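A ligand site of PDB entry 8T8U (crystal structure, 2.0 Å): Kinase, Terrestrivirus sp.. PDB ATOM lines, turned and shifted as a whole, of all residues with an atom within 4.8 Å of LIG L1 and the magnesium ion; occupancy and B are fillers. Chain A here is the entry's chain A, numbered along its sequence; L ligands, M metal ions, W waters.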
ATOM      1  N   PHE A  52     -35.924  -4.309  21.091  1.00  0.00           N
ATOM      2  CA  PHE A  52     -34.999  -5.010  20.166  1.00  0.00           C
ATOM      3  C   PHE A  52     -34.134  -5.970  20.973  1.00  0.00           C
ATOM      4  O   PHE A  52     -33.614  -5.588  22.025  1.00  0.00           O
ATOM      5  CB  PHE A  52     -34.144  -4.030  19.357  1.00  0.00           C
ATOM      6  CG  PHE A  52     -33.296  -4.694  18.313  1.00  0.00           C
ATOM      7  CD1 PHE A  52     -33.836  -5.112  17.105  1.00  0.00           C
ATOM      8  CD2 PHE A  52     -31.949  -4.949  18.557  1.00  0.00           C
ATOM      9  CE1 PHE A  52     -33.054  -5.736  16.154  1.00  0.00           C
ATOM     10  CE2 PHE A  52     -31.164  -5.568  17.594  1.00  0.00           C
ATOM     11  CZ  PHE A  52     -31.717  -5.978  16.402  1.00  0.00           C
ATOM     12  N   ARG A  54     -31.165  -6.901  21.904  1.00  0.00           N
ATOM     13  CA  ARG A  54     -29.734  -6.534  22.039  1.00  0.00           C
ATOM     14  C   ARG A  54     -28.931  -7.733  22.557  1.00  0.00           C
ATOM     15  O   ARG A  54     -29.388  -8.384  23.516  1.00  0.00           O
ATOM     16  CB  ARG A  54     -29.553  -5.391  23.048  1.00  0.00           C
ATOM     17  CG  ARG A  54     -29.954  -4.009  22.539  1.00  0.00           C
ATOM     18  CD  ARG A  54     -30.063  -2.997  23.666  1.00  0.00           C
ATOM     19  NE  ARG A  54     -29.225  -3.325  24.814  1.00  0.00           N
ATOM     20  CZ  ARG A  54     -29.630  -3.382  26.084  1.00  0.00           C
ATOM     21  NH1 ARG A  54     -30.871  -3.087  26.425  1.00  0.00           N
ATOM     22  NH2 ARG A  54     -28.757  -3.712  27.030  1.00  0.00           N
ATOM     23  N   ILE A  55     -27.757  -7.988  21.978  1.00  0.00           N
ATOM     24  CA  ILE A  55     -26.878  -9.096  22.463  1.00  0.00           C
ATOM     25  C   ILE A  55     -25.971  -8.561  23.572  1.00  0.00           C
ATOM     26  O   ILE A  55     -25.488  -9.372  24.367  1.00  0.00           O
ATOM     27  CB  ILE A  55     -26.123  -9.731  21.279  1.00  0.00           C
ATOM     28  CG1 ILE A  55     -26.139 -11.264  21.393  1.00  0.00           C
ATOM     29  CG2 ILE A  55     -24.714  -9.180  21.131  1.00  0.00           C
ATOM     30  CD1 ILE A  55     -27.533 -11.844  21.363  1.00  0.00           C
ATOM     31  N   ALA A  56     -25.770  -7.239  23.642  1.00  0.00           N
ATOM     32  CA  ALA A  56     -24.944  -6.560  24.656  1.00  0.00           C
ATOM     33  C   ALA A  56     -25.352  -5.093  24.779  1.00  0.00           C
ATOM     34  O   ALA A  56     -26.342  -4.698  24.141  1.00  0.00           O
ATOM     35  CB  ALA A  56     -23.485  -6.698  24.298  1.00  0.00           C
ATOM     36  N   GLY A  57     -24.619  -4.319  25.585  1.00  0.00           N
ATOM     37  CA  GLY A  57     -24.817  -2.871  25.755  1.00  0.00           C
ATOM     38  C   GLY A  57     -25.805  -2.564  26.857  1.00  0.00           C
ATOM     39  O   GLY A  57     -26.089  -3.474  27.656  1.00  0.00           O
ATOM     40  N   ARG A  58     -26.333  -1.333  26.881  1.00  0.00           N
ATOM     41  CA  ARG A  58     -27.216  -0.807  27.950  1.00  0.00           C
ATOM     42  C   ARG A  58     -28.285   0.141  27.386  1.00  0.00           C
ATOM     43  O   ARG A  58     -29.288   0.367  28.093  1.00  0.00           O
ATOM     44  CB  ARG A  58     -26.384  -0.035  28.985  1.00  0.00           C
ATOM     45  CG  ARG A  58     -26.053   1.395  28.561  1.00  0.00           C
ATOM     46  CD  ARG A  58     -24.852   1.988  29.278  1.00  0.00           C
ATOM     47  NE  ARG A  58     -23.631   1.256  28.992  1.00  0.00           N
ATOM     48  CZ  ARG A  58     -23.069   0.341  29.796  1.00  0.00           C
ATOM     49  NH1 ARG A  58     -21.960  -0.268  29.408  1.00  0.00           N
ATOM     50  NH2 ARG A  58     -23.608   0.031  30.965  1.00  0.00           N
ATOM     51  N   SER A  59     -28.062   0.726  26.205  1.00  0.00           N
ATOM     52  CA  SER A  59     -28.942   1.755  25.590  1.00  0.00           C
ATOM     53  C   SER A  59     -30.314   1.145  25.277  1.00  0.00           C
ATOM     54  O   SER A  59     -30.382  -0.061  24.947  1.00  0.00           O
ATOM     55  CB  SER A  59     -28.320   2.354  24.355  1.00  0.00           C
ATOM     56  OG  SER A  59     -27.126   3.073  24.678  1.00  0.00           O
ATOM     57  N   ILE A  61     -33.024   0.344  22.896  1.00  0.00           N
ATOM     58  CA  ILE A  61     -33.138   0.068  21.433  1.00  0.00           C
ATOM     59  C   ILE A  61     -34.426  -0.720  21.187  1.00  0.00           C
ATOM     60  O   ILE A  61     -34.587  -1.798  21.772  1.00  0.00           O
ATOM     61  CB  ILE A  61     -31.904  -0.672  20.900  1.00  0.00           C
ATOM     62  CG1 ILE A  61     -30.616   0.105  21.196  1.00  0.00           C
ATOM     63  CG2 ILE A  61     -32.061  -0.966  19.413  1.00  0.00           C
ATOM     64  CD1 ILE A  61     -29.346  -0.587  20.758  1.00  0.00           C
ATOM     65  N   ILE A  70     -34.082   0.043  13.299  1.00  0.00           N
ATOM     66  CA  ILE A  70     -34.075   0.077  14.793  1.00  0.00           C
ATOM     67  C   ILE A  70     -33.931   1.526  15.215  1.00  0.00           C
ATOM     68  O   ILE A  70     -33.287   2.314  14.465  1.00  0.00           O
ATOM     69  CB  ILE A  70     -32.990  -0.824  15.393  1.00  0.00           C
ATOM     70  CG1 ILE A  70     -31.578  -0.412  14.939  1.00  0.00           C
ATOM     71  CG2 ILE A  70     -33.284  -2.286  15.072  1.00  0.00           C
ATOM     72  CD1 ILE A  70     -30.480  -0.976  15.807  1.00  0.00           C
ATOM     73  N   LYS A  72     -32.399   3.721  18.280  1.00  0.00           N
ATOM     74  CA  LYS A  72     -31.468   3.701  19.440  1.00  0.00           C
ATOM     75  C   LYS A  72     -31.572   5.050  20.132  1.00  0.00           C
ATOM     76  O   LYS A  72     -31.342   6.074  19.457  1.00  0.00           O
ATOM     77  CB  LYS A  72     -30.029   3.425  18.995  1.00  0.00           C
ATOM     78  CG  LYS A  72     -29.007   3.492  20.122  1.00  0.00           C
ATOM     79  CD  LYS A  72     -27.574   3.300  19.700  1.00  0.00           C
ATOM     80  CE  LYS A  72     -26.617   3.495  20.853  1.00  0.00           C
ATOM     81  NZ  LYS A  72     -25.205   3.309  20.437  1.00  0.00           N
ATOM     82  N   GLU A  80     -23.041  10.785  19.541  1.00  0.00           N
ATOM     83  CA  GLU A  80     -23.139   9.727  18.505  1.00  0.00           C
ATOM     84  C   GLU A  80     -23.640  10.351  17.196  1.00  0.00           C
ATOM     85  O   GLU A  80     -23.058  10.049  16.138  1.00  0.00           O
ATOM     86  CB  GLU A  80     -24.009   8.557  18.955  1.00  0.00           C
ATOM     87  CG  GLU A  80     -23.993   7.429  17.956  1.00  0.00           C
ATOM     88  CD  GLU A  80     -24.333   6.054  18.498  1.00  0.00           C
ATOM     89  OE1 GLU A  80     -25.162   5.973  19.428  1.00  0.00           O
ATOM     90  OE2 GLU A  80     -23.759   5.065  17.982  1.00  0.00           O
ATOM     91  N   PRO A 100     -23.641   0.796   9.903  1.00  0.00           N
ATOM     92  CA  PRO A 100     -25.055   0.755   9.547  1.00  0.00           C
ATOM     93  C   PRO A 100     -25.493   2.143   9.056  1.00  0.00           C
ATOM     94  O   PRO A 100     -25.028   3.133   9.584  1.00  0.00           O
ATOM     95  CB  PRO A 100     -25.789   0.380  10.842  1.00  0.00           C
ATOM     96  CG  PRO A 100     -24.769   0.609  11.945  1.00  0.00           C
ATOM     97  CD  PRO A 100     -23.414   0.395  11.305  1.00  0.00           C
ATOM     98  N   LEU A 112     -31.599   3.755  12.653  1.00  0.00           N
ATOM     99  CA  LEU A 112     -30.437   3.020  12.091  1.00  0.00           C
ATOM    100  C   LEU A 112     -30.942   1.828  11.302  1.00  0.00           C
ATOM    101  O   LEU A 112     -32.004   1.280  11.642  1.00  0.00           O
ATOM    102  CB  LEU A 112     -29.516   2.554  13.220  1.00  0.00           C
ATOM    103  CG  LEU A 112     -28.823   3.645  14.028  1.00  0.00           C
ATOM    104  CD1 LEU A 112     -28.039   3.033  15.180  1.00  0.00           C
ATOM    105  CD2 LEU A 112     -27.899   4.484  13.165  1.00  0.00           C
ATOM    106  N   GLU A 113     -30.157   1.417  10.316  1.00  0.00           N
ATOM    107  CA  GLU A 113     -30.309   0.129   9.598  1.00  0.00           C
ATOM    108  C   GLU A 113     -30.230  -1.001  10.633  1.00  0.00           C
ATOM    109  O   GLU A 113     -29.271  -1.029  11.433  1.00  0.00           O
ATOM    110  CB  GLU A 113     -29.212   0.057   8.531  1.00  0.00           C
ATOM    111  CG  GLU A 113     -29.068  -1.300   7.875  1.00  0.00           C
ATOM    112  CD  GLU A 113     -27.834  -1.437   6.990  1.00  0.00           C
ATOM    113  OE1 GLU A 113     -27.058  -0.461   6.887  1.00  0.00           O
ATOM    114  OE2 GLU A 113     -27.644  -2.532   6.435  1.00  0.00           O
ATOM    115  N   ASP A 114     -31.233  -1.892  10.633  1.00  0.00           N
ATOM    116  CA  ASP A 114     -31.246  -3.158  11.404  1.00  0.00           C
ATOM    117  C   ASP A 114     -30.312  -4.156  10.716  1.00  0.00           C
ATOM    118  O   ASP A 114     -30.698  -4.716   9.666  1.00  0.00           O
ATOM    119  CB  ASP A 114     -32.657  -3.739  11.517  1.00  0.00           C
ATOM    120  CG  ASP A 114     -32.741  -5.071  12.263  1.00  0.00           C
ATOM    121  OD1 ASP A 114     -31.672  -5.591  12.678  1.00  0.00           O
ATOM    122  OD2 ASP A 114     -33.872  -5.576  12.412  1.00  0.00           O
ATOM    123  N   LEU A 115     -29.134  -4.398  11.299  1.00  0.00           N
ATOM    124  CA  LEU A 115     -28.099  -5.281  10.707  1.00  0.00           C
ATOM    125  C   LEU A 115     -28.575  -6.742  10.709  1.00  0.00           C
ATOM    126  O   LEU A 115     -27.957  -7.541   9.996  1.00  0.00           O
ATOM    127  CB  LEU A 115     -26.780  -5.105  11.478  1.00  0.00           C
ATOM    128  CG  LEU A 115     -26.108  -3.752  11.324  1.00  0.00           C
ATOM    129  CD1 LEU A 115     -24.902  -3.642  12.230  1.00  0.00           C
ATOM    130  CD2 LEU A 115     -25.691  -3.504   9.881  1.00  0.00           C
ATOM    131  N   THR A 116     -29.616  -7.095  11.467  1.00  0.00           N
ATOM    132  CA  THR A 116     -30.138  -8.485  11.555  1.00  0.00           C
ATOM    133  C   THR A 116     -31.271  -8.693  10.551  1.00  0.00           C
ATOM    134  O   THR A 116     -31.744  -9.844  10.431  1.00  0.00           O
ATOM    135  CB  THR A 116     -30.606  -8.841  12.970  1.00  0.00           C
ATOM    136  OG1 THR A 116     -31.730  -8.028  13.330  1.00  0.00           O
ATOM    137  CG2 THR A 116     -29.531  -8.676  14.014  1.00  0.00           C
ATOM    138  N   VAL A 124     -25.285 -13.311  16.438  1.00  0.00           N
ATOM    139  CA  VAL A 124     -24.703 -11.955  16.628  1.00  0.00           C
ATOM    140  C   VAL A 124     -23.641 -12.020  17.730  1.00  0.00           C
ATOM    141  O   VAL A 124     -23.926 -12.627  18.781  1.00  0.00           O
ATOM    142  CB  VAL A 124     -25.799 -10.923  16.969  1.00  0.00           C
ATOM    143  CG1 VAL A 124     -25.218  -9.534  17.140  1.00  0.00           C
ATOM    144  CG2 VAL A 124     -26.902 -10.930  15.931  1.00  0.00           C
ATOM    145  N   ASP A 126     -20.975  -9.149  19.685  1.00  0.00           N
ATOM    146  CA  ASP A 126     -20.536  -7.759  19.918  1.00  0.00           C
ATOM    147  C   ASP A 126     -19.129  -7.830  20.499  1.00  0.00           C
ATOM    148  O   ASP A 126     -18.976  -8.425  21.596  1.00  0.00           O
ATOM    149  CB  ASP A 126     -21.528  -7.018  20.835  1.00  0.00           C
ATOM    150  CG  ASP A 126     -21.134  -5.604  21.206  1.00  0.00           C
ATOM    151  OD1 ASP A 126     -19.912  -5.341  21.333  1.00  0.00           O
ATOM    152  OD2 ASP A 126     -22.042  -4.778  21.387  1.00  0.00           O
ATOM    153  N   LYS A 128     -16.068  -5.248  21.544  1.00  0.00           N
ATOM    154  CA  LYS A 128     -15.623  -3.856  21.818  1.00  0.00           C
ATOM    155  C   LYS A 128     -14.147  -3.768  21.410  1.00  0.00           C
ATOM    156  O   LYS A 128     -13.323  -4.484  22.023  1.00  0.00           O
ATOM    157  CB  LYS A 128     -15.917  -3.547  23.289  1.00  0.00           C
ATOM    158  CG  LYS A 128     -15.227  -2.331  23.874  1.00  0.00           C
ATOM    159  CD  LYS A 128     -16.085  -1.113  23.944  1.00  0.00           C
ATOM    160  CE  LYS A 128     -17.266  -1.232  24.890  1.00  0.00           C
ATOM    161  NZ  LYS A 128     -18.186  -0.081  24.698  1.00  0.00           N
ATOM    162  N   GLY A 211     -14.808   3.136  22.651  1.00  0.00           N
ATOM    163  CA  GLY A 211     -16.076   2.453  22.973  1.00  0.00           C
ATOM    164  C   GLY A 211     -16.738   1.772  21.778  1.00  0.00           C
ATOM    165  O   GLY A 211     -17.802   1.161  22.002  1.00  0.00           O
ATOM    166  N   SER A 213     -17.813  -0.925  18.903  1.00  0.00           N
ATOM    167  CA  SER A 213     -17.913  -2.399  18.805  1.00  0.00           C
ATOM    168  C   SER A 213     -17.976  -2.816  17.331  1.00  0.00           C
ATOM    169  O   SER A 213     -18.477  -2.038  16.496  1.00  0.00           O
ATOM    170  CB  SER A 213     -19.109  -2.930  19.546  1.00  0.00           C
ATOM    171  OG  SER A 213     -18.875  -2.914  20.945  1.00  0.00           O
ATOM    172  N   ILE A 215     -19.913  -5.662  15.259  1.00  0.00           N
ATOM    173  CA  ILE A 215     -21.098  -6.559  15.319  1.00  0.00           C
ATOM    174  C   ILE A 215     -20.926  -7.602  14.209  1.00  0.00           C
ATOM    175  O   ILE A 215     -21.103  -7.232  13.037  1.00  0.00           O
ATOM    176  CB  ILE A 215     -22.413  -5.768  15.198  1.00  0.00           C
ATOM    177  CG1 ILE A 215     -22.464  -4.615  16.198  1.00  0.00           C
ATOM    178  CG2 ILE A 215     -23.616  -6.684  15.315  1.00  0.00           C
ATOM    179  CD1 ILE A 215     -22.241  -5.018  17.630  1.00  0.00           C
ATOM    180  N   VAL A 230     -20.213  -0.139  15.188  1.00  0.00           N
ATOM    181  CA  VAL A 230     -21.337   0.593  15.850  1.00  0.00           C
ATOM    182  C   VAL A 230     -20.849   1.254  17.131  1.00  0.00           C
ATOM    183  O   VAL A 230     -19.720   0.929  17.602  1.00  0.00           O
ATOM    184  CB  VAL A 230     -22.529  -0.344  16.132  1.00  0.00           C
ATOM    185  CG1 VAL A 230     -22.948  -1.113  14.880  1.00  0.00           C
ATOM    186  CG2 VAL A 230     -22.223  -1.309  17.278  1.00  0.00           C
ATOM    187  N   ASP A 231     -21.697   2.137  17.670  1.00  0.00           N
ATOM    188  CA  ASP A 231     -21.592   2.804  18.993  1.00  0.00           C
ATOM    189  C   ASP A 231     -20.510   3.879  18.909  1.00  0.00           C
ATOM    190  O   ASP A 231     -19.367   3.619  19.331  1.00  0.00           O
ATOM    191  CB  ASP A 231     -21.323   1.803  20.125  1.00  0.00           C
ATOM    192  CG  ASP A 231     -21.569   2.404  21.500  1.00  0.00           C
ATOM    193  OD1 ASP A 231     -21.723   3.642  21.585  1.00  0.00           O
ATOM    194  OD2 ASP A 231     -21.596   1.628  22.482  1.00  0.00           O
HETATM  195  P1  LIG L   1     -24.852   0.542  23.707  1.00  0.00           P
HETATM  196  O1  LIG L   1     -23.535  -0.143  23.976  1.00  0.00           O
HETATM  197  O2  LIG L   1     -26.005  -0.116  24.410  1.00  0.00           O
HETATM  198  O3  LIG L   1     -24.793   2.031  23.933  1.00  0.00           O
HETATM  199  P2  LIG L   1     -24.423  -0.248  20.843  1.00  0.00           P
HETATM  200  O4  LIG L   1     -23.076  -0.721  21.260  1.00  0.00           O
HETATM  201  O5  LIG L   1     -24.539   0.758  19.731  1.00  0.00           O
HETATM  202  O6  LIG L   1     -25.185   0.383  22.117  1.00  0.00           O
HETATM  203  O7  LIG L   1     -25.354  -1.510  20.505  1.00  0.00           O
HETATM  204  C1  LIG L   1     -25.650  -2.444  21.569  1.00  0.00           C
HETATM  205  C2  LIG L   1     -26.201  -3.718  20.970  1.00  0.00           C
HETATM  206  O8  LIG L   1     -27.333  -3.387  20.130  1.00  0.00           O
HETATM  207  C3  LIG L   1     -25.236  -4.503  20.069  1.00  0.00           C
HETATM  208  O9  LIG L   1     -24.494  -5.453  20.829  1.00  0.00           O
HETATM  209  C4  LIG L   1     -26.196  -5.185  19.094  1.00  0.00           C
HETATM  210  O10 LIG L   1     -26.697  -6.390  19.649  1.00  0.00           O
HETATM  211  C5  LIG L   1     -27.312  -4.153  18.944  1.00  0.00           C
HETATM  212  N1  LIG L   1     -27.179  -3.233  17.816  1.00  0.00           N
HETATM  213  C6  LIG L   1     -26.684  -1.953  17.812  1.00  0.00           C
HETATM  214  N2  LIG L   1     -26.762  -1.356  16.647  1.00  0.00           N
HETATM  215  C7  LIG L   1     -27.360  -2.290  15.825  1.00  0.00           C
HETATM  216  C8  LIG L   1     -27.733  -2.263  14.474  1.00  0.00           C
HETATM  217  N3  LIG L   1     -27.567  -1.208  13.681  1.00  0.00           N
HETATM  218  N4  LIG L   1     -28.352  -3.366  13.963  1.00  0.00           N
HETATM  219  C9  LIG L   1     -28.534  -4.422  14.768  1.00  0.00           C
HETATM  220  N5  LIG L   1     -28.211  -4.563  16.057  1.00  0.00           N
HETATM  221  C10 LIG L   1     -27.632  -3.452  16.532  1.00  0.00           C
HETATM  222  P1  LG2 L   2     -21.012  -1.374  25.899  1.00  0.00           P
HETATM  223  O1  LG2 L   2     -20.687  -0.550  24.646  1.00  0.00           O
HETATM  224  O2  LG2 L   2     -22.398  -0.938  26.408  1.00  0.00           O
HETATM  225  O3  LG2 L   2     -19.969  -1.110  26.982  1.00  0.00           O
HETATM  226  O4  LG2 L   2     -21.014  -2.871  25.568  1.00  0.00           O
HETATM  227 MG    MG M   1     -21.828  -0.520  22.796  1.00  0.00          MG
HETATM  228  O   HOH W   1     -25.740   1.235  17.258  1.00  0.00           O
HETATM  229  O   HOH W   2     -21.822   2.872  24.821  1.00  0.00           O
HETATM  230  O   HOH W   3     -23.245   1.473  26.451  1.00  0.00           O
HETATM  231  O   HOH W   4     -21.849  -2.715  23.092  1.00  0.00           O
HETATM  232  O   HOH W   5     -28.041  -7.206  17.429  1.00  0.00           O
HETATM  233  O   HOH W   6     -23.813   4.061  23.036  1.00  0.00           O
HETATM  234  O   HOH W   7     -19.944  -0.757  21.978  1.00  0.00           O
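The guanidinium group (NH1) of Arg 54 sits close to the backbone carbonyl oxygen (O) of Ser 59 (3.4 Å).
The side-chain carboxylate of Glu 80 is in salt-bridge range of the side-chain amino group of Lys 72, at 2.8 Å.
The backbone carbonyl oxygen (O) of Gly 57 lies within hydrogen-bond range of the guanidinium group (NH2) of Arg 54 (2.8 Å).
The backbone NH (N) of Leu 112 lies within hydrogen-bond range of the backbone carbonyl oxygen (O) of Ile 70.
The guanidinium group of Arg 54 sits at hydrogen-bond distance from the backbone carbonyl oxygen of Ala 56, 3.3 Å away.
N of Phe 52 lies within hydrogen-bond range of O of Ile 61 (2.9 Å).
The side-chain carboxylate (OD1) of Asp 114 sits at hydrogen-bond distance from the side-chain hydroxyl (OG1) of Thr 116 (2.5 Å).
The backbone NH (N) of Val 230 sits at hydrogen-bond distance from the backbone carbonyl oxygen (O) of Ser 213.
Water W7 lies within hydrogen-bond range of OG of Ser 213 (2.6 Å), O of Gly 211 (2.9 Å) and NZ of Lys 128 (3.3 Å).
Water W6 lies within hydrogen-bond range of an oxygen (O3) of LIG L1 (2.4 Å), the side-chain carboxylate of Asp 231 (2.6 Å) and the side-chain amino group of Lys 72 (3.0 Å).
Water W3 lies within hydrogen-bond range of the guanidinium group of Arg 58 (2.6 Å) and an oxygen (O3) of LIG L1 (3.0 Å).
Water W2 lies within hydrogen-bond range of an oxygen (O3) of LIG L1 (3.2 Å) and the side-chain carboxylate of Asp 231 (3.3 Å).
The side-chain carboxylate of Asp 126 lies within hydrogen-bond range of an oxygen (O9) of LIG L1, 2.6 Å away.
O2 of LIG L1 is in hydrogen-bond range of N of Ser 59 (2.9 Å).
The side-chain hydroxyl of Ser 59 is in hydrogen-bond range of an oxygen (O3) of LIG L1, 2.7 Å away.
The side-chain amino group (NZ) of Lys 72 lies within salt-bridge range of an oxygen (O5) of LIG L1, 2.7 Å away.
O2 of LIG L1 is in hydrogen-bond range of N of Arg 58, 2.8 Å away.
The backbone carbonyl oxygen of Glu 113 lies within hydrogen-bond range of a nitrogen (N3) of LIG L1 (2.8 Å).
The backbone NH (N) of Leu 115 lies within hydrogen-bond range of a nitrogen (N4) of LIG L1, 3.0 Å away.
The backbone NH of Ile 55 sits at hydrogen-bond distance from an oxygen (O10) of LIG L1, at 3.0 Å.
The magnesium ion is bound by O4 of LIG L1 (2.0 Å), water W7 (2.1 Å), O1 of LIG L1 (2.1 Å), O1 of LG2 L2 (2.2 Å), OD2 of Asp 231 (2.2 Å) and water W4 (2.2 Å).
The magnesium ion has six donor atoms within binding distance.
One residue has an atom within 4 Å of the magnesium ion: Asp 231.
The nearest printed residue that does not touch the magnesium ion is Lys 128 (4.1 Å).
Residues that only touch LIG L1: Gly 57, Ile 70, Ala 56, Phe 52, Ile 61, Arg 54, Pro 100, Asp 114, Ile 215 and Val 230.
Hydrophobic or aromatic side chains that line LIG L1: Phe 52, Ile 55, Ala 56, Ile 61, Ile 70, Pro 100, Leu 115, Ile 215 and Val 230.
Within 4 Å of LIG L1: Phe 52, Arg 54, Ile 55, Ala 56, Gly 57, Arg 58, Ser 59, Ile 61, Ile 70, Lys 72, Pro 100, Glu 113, Asp 114, Leu 115, Asp 126, Ile 215, Val 230 and Asp 231.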
